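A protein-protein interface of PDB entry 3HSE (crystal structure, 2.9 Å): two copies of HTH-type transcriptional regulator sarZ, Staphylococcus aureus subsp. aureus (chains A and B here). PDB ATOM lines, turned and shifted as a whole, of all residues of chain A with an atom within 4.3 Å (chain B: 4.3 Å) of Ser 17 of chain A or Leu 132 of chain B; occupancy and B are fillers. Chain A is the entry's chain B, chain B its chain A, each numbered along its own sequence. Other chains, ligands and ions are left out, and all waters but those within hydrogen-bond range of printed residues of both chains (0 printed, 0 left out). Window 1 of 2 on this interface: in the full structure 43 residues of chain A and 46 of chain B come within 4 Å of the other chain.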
ATOM      1  N   LEU A  13      -7.572  14.174   0.095  1.00  0.00           N
ATOM      2  CA  LEU A  13      -6.934  15.082   1.037  1.00  0.00           C
ATOM      3  C   LEU A  13      -6.486  14.444   2.321  1.00  0.00           C
ATOM      4  O   LEU A  13      -5.404  14.741   2.819  1.00  0.00           O
ATOM      5  CB  LEU A  13      -7.861  16.244   1.371  1.00  0.00           C
ATOM      6  CG  LEU A  13      -7.981  17.376   0.351  1.00  0.00           C
ATOM      7  CD1 LEU A  13      -8.832  18.468   0.957  1.00  0.00           C
ATOM      8  CD2 LEU A  13      -6.589  17.910  -0.021  1.00  0.00           C
ATOM      9  N   PHE A  14      -7.325  13.580   2.879  1.00  0.00           N
ATOM     10  CA  PHE A  14      -6.954  12.901   4.113  1.00  0.00           C
ATOM     11  C   PHE A  14      -5.783  11.952   3.806  1.00  0.00           C
ATOM     12  O   PHE A  14      -4.817  11.861   4.572  1.00  0.00           O
ATOM     13  CB  PHE A  14      -8.162  12.143   4.702  1.00  0.00           C
ATOM     14  CG  PHE A  14      -8.901  12.912   5.799  1.00  0.00           C
ATOM     15  CD1 PHE A  14      -8.265  13.224   7.007  1.00  0.00           C
ATOM     16  CD2 PHE A  14     -10.233  13.313   5.626  1.00  0.00           C
ATOM     17  CE1 PHE A  14      -8.938  13.927   8.026  1.00  0.00           C
ATOM     18  CE2 PHE A  14     -10.923  14.018   6.639  1.00  0.00           C
ATOM     19  CZ  PHE A  14     -10.275  14.324   7.840  1.00  0.00           C
ATOM     20  N   TYR A  15      -5.853  11.275   2.666  1.00  0.00           N
ATOM     21  CA  TYR A  15      -4.799  10.358   2.287  1.00  0.00           C
ATOM     22  C   TYR A  15      -3.450  11.061   2.131  1.00  0.00           C
ATOM     23  O   TYR A  15      -2.464  10.726   2.806  1.00  0.00           O
ATOM     24  CB  TYR A  15      -5.142   9.684   0.976  1.00  0.00           C
ATOM     25  CG  TYR A  15      -4.070   8.715   0.541  1.00  0.00           C
ATOM     26  CD1 TYR A  15      -3.962   7.457   1.140  1.00  0.00           C
ATOM     27  CD2 TYR A  15      -3.135   9.065  -0.442  1.00  0.00           C
ATOM     28  CE1 TYR A  15      -2.956   6.570   0.775  1.00  0.00           C
ATOM     29  CE2 TYR A  15      -2.119   8.182  -0.814  1.00  0.00           C
ATOM     30  CZ  TYR A  15      -2.036   6.936  -0.202  1.00  0.00           C
ATOM     31  OH  TYR A  15      -1.040   6.048  -0.560  1.00  0.00           O
ATOM     32  N   VAL A  16      -3.416  12.033   1.226  1.00  0.00           N
ATOM     33  CA  VAL A  16      -2.204  12.790   0.938  1.00  0.00           C
ATOM     34  C   VAL A  16      -1.659  13.590   2.119  1.00  0.00           C
ATOM     35  O   VAL A  16      -0.516  13.388   2.525  1.00  0.00           O
ATOM     36  CB  VAL A  16      -2.427  13.745  -0.262  1.00  0.00           C
ATOM     37  CG1 VAL A  16      -1.230  14.650  -0.438  1.00  0.00           C
ATOM     38  CG2 VAL A  16      -2.670  12.933  -1.527  1.00  0.00           C
ATOM     39  N   SER A  17      -2.466  14.492   2.675  1.00  0.00           N
ATOM     40  CA  SER A  17      -2.007  15.311   3.796  1.00  0.00           C
ATOM     41  C   SER A  17      -1.344  14.474   4.883  1.00  0.00           C
ATOM     42  O   SER A  17      -0.255  14.804   5.336  1.00  0.00           O
ATOM     43  CB  SER A  17      -3.162  16.108   4.405  1.00  0.00           C
ATOM     44  OG  SER A  17      -4.024  15.267   5.140  1.00  0.00           O
ATOM     45  N   SER A  18      -1.983  13.391   5.302  1.00  0.00           N
ATOM     46  CA  SER A  18      -1.394  12.557   6.342  1.00  0.00           C
ATOM     47  C   SER A  18      -0.280  11.677   5.751  1.00  0.00           C
ATOM     48  O   SER A  18       0.597  11.166   6.470  1.00  0.00           O
ATOM     49  CB  SER A  18      -2.477  11.686   7.004  1.00  0.00           C
ATOM     50  OG  SER A  18      -2.636  10.448   6.338  1.00  0.00           O
ATOM     51  N   LYS A  19      -0.313  11.503   4.435  1.00  0.00           N
ATOM     52  CA  LYS A  19       0.695  10.698   3.760  1.00  0.00           C
ATOM     53  C   LYS A  19       2.040  11.439   3.848  1.00  0.00           C
ATOM     54  O   LYS A  19       3.082  10.827   4.059  1.00  0.00           O
ATOM     55  CB  LYS A  19       0.265  10.460   2.306  1.00  0.00           C
ATOM     56  CG  LYS A  19       0.939   9.287   1.621  1.00  0.00           C
ATOM     57  CD  LYS A  19       0.779   7.990   2.395  1.00  0.00           C
ATOM     58  CE  LYS A  19       1.478   6.850   1.664  1.00  0.00           C
ATOM     59  NZ  LYS A  19       1.815   5.666   2.525  1.00  0.00           N
ATOM     60  N   GLU A  20       1.992  12.763   3.715  1.00  0.00           N
ATOM     61  CA  GLU A  20       3.172  13.625   3.793  1.00  0.00           C
ATOM     62  C   GLU A  20       3.577  13.990   5.220  1.00  0.00           C
ATOM     63  O   GLU A  20       4.695  14.452   5.461  1.00  0.00           O
ATOM     64  CB  GLU A  20       2.924  14.917   3.045  1.00  0.00           C
ATOM     65  CG  GLU A  20       2.833  14.743   1.568  1.00  0.00           C
ATOM     66  CD  GLU A  20       2.519  16.042   0.882  1.00  0.00           C
ATOM     67  OE1 GLU A  20       1.527  16.690   1.284  1.00  0.00           O
ATOM     68  OE2 GLU A  20       3.260  16.418  -0.052  1.00  0.00           O
ATOM     69  N   ILE A  21       2.651  13.812   6.155  1.00  0.00           N
ATOM     70  CA  ILE A  21       2.909  14.099   7.553  1.00  0.00           C
ATOM     71  C   ILE A  21       3.787  12.981   8.075  1.00  0.00           C
ATOM     72  O   ILE A  21       4.814  13.227   8.707  1.00  0.00           O
ATOM     73  CB  ILE A  21       1.586  14.199   8.328  1.00  0.00           C
ATOM     74  CG1 ILE A  21       0.976  15.582   8.047  1.00  0.00           C
ATOM     75  CG2 ILE A  21       1.808  13.969   9.798  1.00  0.00           C
ATOM     76  CD1 ILE A  21      -0.366  15.867   8.675  1.00  0.00           C
ATOM     77  N   PHE B  14      -4.503  13.707  13.871  1.00  0.00           N
ATOM     78  CA  PHE B  14      -4.320  13.268  12.496  1.00  0.00           C
ATOM     79  C   PHE B  14      -4.172  11.769  12.486  1.00  0.00           C
ATOM     80  O   PHE B  14      -4.742  11.095  11.642  1.00  0.00           O
ATOM     81  CB  PHE B  14      -3.077  13.897  11.871  1.00  0.00           C
ATOM     82  CG  PHE B  14      -3.334  15.211  11.195  1.00  0.00           C
ATOM     83  CD1 PHE B  14      -4.086  15.267  10.015  1.00  0.00           C
ATOM     84  CD2 PHE B  14      -2.813  16.398  11.719  1.00  0.00           C
ATOM     85  CE1 PHE B  14      -4.310  16.495   9.362  1.00  0.00           C
ATOM     86  CE2 PHE B  14      -3.027  17.633  11.073  1.00  0.00           C
ATOM     87  CZ  PHE B  14      -3.776  17.684   9.895  1.00  0.00           C
ATOM     88  N   ILE B 128     -12.665  21.132   6.556  1.00  0.00           N
ATOM     89  CA  ILE B 128     -11.606  20.155   6.668  1.00  0.00           C
ATOM     90  C   ILE B 128     -10.770  20.202   5.400  1.00  0.00           C
ATOM     91  O   ILE B 128      -9.541  20.107   5.455  1.00  0.00           O
ATOM     92  CB  ILE B 128     -12.195  18.747   6.921  1.00  0.00           C
ATOM     93  CG1 ILE B 128     -13.012  18.765   8.219  1.00  0.00           C
ATOM     94  CG2 ILE B 128     -11.084  17.723   7.054  1.00  0.00           C
ATOM     95  CD1 ILE B 128     -13.862  17.556   8.420  1.00  0.00           C
ATOM     96  N   ILE B 129     -11.433  20.387   4.262  1.00  0.00           N
ATOM     97  CA  ILE B 129     -10.738  20.482   2.978  1.00  0.00           C
ATOM     98  C   ILE B 129      -9.888  21.772   2.892  1.00  0.00           C
ATOM     99  O   ILE B 129      -8.779  21.767   2.327  1.00  0.00           O
ATOM    100  CB  ILE B 129     -11.750  20.444   1.790  1.00  0.00           C
ATOM    101  CG1 ILE B 129     -12.458  19.087   1.752  1.00  0.00           C
ATOM    102  CG2 ILE B 129     -11.027  20.661   0.465  1.00  0.00           C
ATOM    103  CD1 ILE B 129     -13.508  18.965   0.653  1.00  0.00           C
ATOM    104  N   ASN B 130     -10.403  22.876   3.442  1.00  0.00           N
ATOM    105  CA  ASN B 130      -9.651  24.130   3.418  1.00  0.00           C
ATOM    106  C   ASN B 130      -8.402  23.995   4.285  1.00  0.00           C
ATOM    107  O   ASN B 130      -7.343  24.538   3.957  1.00  0.00           O
ATOM    108  CB  ASN B 130     -10.513  25.299   3.905  1.00  0.00           C
ATOM    109  CG  ASN B 130     -11.635  25.650   2.923  1.00  0.00           C
ATOM    110  OD1 ASN B 130     -11.433  25.625   1.704  1.00  0.00           O
ATOM    111  ND2 ASN B 130     -12.816  25.991   3.448  1.00  0.00           N
ATOM    112  N   ASN B 131      -8.541  23.241   5.377  1.00  0.00           N
ATOM    113  CA  ASN B 131      -7.459  22.983   6.326  1.00  0.00           C
ATOM    114  C   ASN B 131      -6.481  21.961   5.770  1.00  0.00           C
ATOM    115  O   ASN B 131      -5.273  22.177   5.766  1.00  0.00           O
ATOM    116  CB  ASN B 131      -8.018  22.432   7.640  1.00  0.00           C
ATOM    117  CG  ASN B 131      -8.713  23.486   8.480  1.00  0.00           C
ATOM    118  OD1 ASN B 131      -9.635  23.175   9.226  1.00  0.00           O
ATOM    119  ND2 ASN B 131      -8.261  24.724   8.384  1.00  0.00           N
ATOM    120  N   LEU B 132      -7.005  20.833   5.313  1.00  0.00           N
ATOM    121  CA  LEU B 132      -6.150  19.788   4.788  1.00  0.00           C
ATOM    122  C   LEU B 132      -5.276  20.178   3.594  1.00  0.00           C
ATOM    123  O   LEU B 132      -4.379  19.426   3.216  1.00  0.00           O
ATOM    124  CB  LEU B 132      -6.995  18.553   4.456  1.00  0.00           C
ATOM    125  CG  LEU B 132      -7.374  17.661   5.650  1.00  0.00           C
ATOM    126  CD1 LEU B 132      -8.315  16.526   5.219  1.00  0.00           C
ATOM    127  CD2 LEU B 132      -6.096  17.104   6.263  1.00  0.00           C
ATOM    128  N   ARG B 133      -5.512  21.350   3.007  1.00  0.00           N
ATOM    129  CA  ARG B 133      -4.709  21.799   1.856  1.00  0.00           C
ATOM    130  C   ARG B 133      -3.307  22.288   2.246  1.00  0.00           C
ATOM    131  O   ARG B 133      -2.327  22.043   1.542  1.00  0.00           O
ATOM    132  CB  ARG B 133      -5.450  22.904   1.093  1.00  0.00           C
ATOM    133  CG  ARG B 133      -6.504  22.370   0.142  1.00  0.00           C
ATOM    134  CD  ARG B 133      -7.480  23.453  -0.277  1.00  0.00           C
ATOM    135  NE  ARG B 133      -8.643  22.895  -0.969  1.00  0.00           N
ATOM    136  CZ  ARG B 133      -9.781  23.554  -1.178  1.00  0.00           C
ATOM    137  NH1 ARG B 133      -9.919  24.802  -0.746  1.00  0.00           N
ATOM    138  NH2 ARG B 133     -10.783  22.962  -1.818  1.00  0.00           N
ATOM    139  N   ASN B 134      -3.213  22.969   3.378  1.00  0.00           N
ATOM    140  CA  ASN B 134      -1.935  23.474   3.856  1.00  0.00           C
ATOM    141  C   ASN B 134      -0.903  22.353   3.920  1.00  0.00           C
ATOM    142  O   ASN B 134       0.286  22.608   4.055  1.00  0.00           O
ATOM    143  CB  ASN B 134      -2.105  24.089   5.249  1.00  0.00           C
ATOM    144  CG  ASN B 134      -3.457  24.780   5.427  1.00  0.00           C
ATOM    145  OD1 ASN B 134      -3.872  25.600   4.601  1.00  0.00           O
ATOM    146  ND2 ASN B 134      -4.145  24.450   6.517  1.00  0.00           N
ATOM    147  N   PHE B 135      -1.365  21.113   3.821  1.00  0.00           N
ATOM    148  CA  PHE B 135      -0.482  19.952   3.881  1.00  0.00           C
ATOM    149  C   PHE B 135      -0.278  19.410   2.483  1.00  0.00           C
ATOM    150  O   PHE B 135       0.019  18.235   2.287  1.00  0.00           O
ATOM    151  CB  PHE B 135      -1.086  18.868   4.789  1.00  0.00           C
ATOM    152  CG  PHE B 135      -1.352  19.341   6.190  1.00  0.00           C
ATOM    153  CD1 PHE B 135      -0.421  19.144   7.193  1.00  0.00           C
ATOM    154  CD2 PHE B 135      -2.502  20.069   6.483  1.00  0.00           C
ATOM    155  CE1 PHE B 135      -0.630  19.668   8.465  1.00  0.00           C
ATOM    156  CE2 PHE B 135      -2.714  20.596   7.748  1.00  0.00           C
ATOM    157  CZ  PHE B 135      -1.777  20.395   8.741  1.00  0.00           C
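The side-chain carboxylate (OE1) of Glu 20 of chain A sits close to the backbone carbonyl oxygen (O) of Phe 135 of chain B.
The backbone carbonyl oxygen (O) of Ile 129 of chain B lies close to the guanidinium group (NE) of Arg 133 of chain B, at 3.5 Å.
The side-chain hydroxyl (OG) of Ser 17 of chain A is in hydrogen-bond range of the backbone carbonyl oxygen (O) of Leu 13 of chain A, 2.8 Å away.
The backbone carbonyl oxygen of Phe 14 of chain A sits at hydrogen-bond distance from the side-chain hydroxyl of Ser 18 of chain A (3.1 Å).
Among the printed residues, pairs that only touch across the chains: Ser 17 of chain A with Leu 132 of chain B, Leu 13 of chain A with Ile 129 of chain B, Ser 17 of chain A with Phe 135 of chain B, Phe 14 of chain A with Ile 128 of chain B, Ile 21 of chain A with Phe 135 of chain B, Phe 14 of chain A with Leu 132 of chain B, Leu 13 of chain A with Leu 132 of chain B and Ile 21 of chain A with Phe 14 of chain B.
Of the printed residues of chain B, Leu 13 of chain A touches Ile 129 and Leu 132.
Ser 17 of chain A touches two residues of chain B.
Of the printed residues of chain B, Glu 20 of chain A touches Phe 135 (2.4 Å).
Of the printed residues of chain B, Ile 21 of chain A touches Phe 14 (3.9 Å) and Phe 135 (3.6 Å).
Asn 130 of chain B touches none of the printed residues of chain A.
Of chain A, only Leu 13 (3.9 Å), Phe 14 (3.7 Å) and Ser 17 (3.0 Å) come within 4 Å of Leu 132 of chain B.
The nearest printed residue of chain B that does not touch Ser 17 of chain A is Phe 14 of chain B (4.4 Å).
The nearest printed residue of chain A that does not touch Ile 128 of chain B is Leu 13 of chain A (4.8 Å).
Hydrophobic or aromatic side chains of chain B within 4 Å of the printed part of chain A: Phe 14, Ile 128, Ile 129, Leu 132 and Phe 135.
Among the printed residues, 9 pairs touch across the chains.
1 position is printed for both chains.
Of the 9 pairs that touch across the chains among the printed residues, none has its exchanged pair printed and touching as well.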
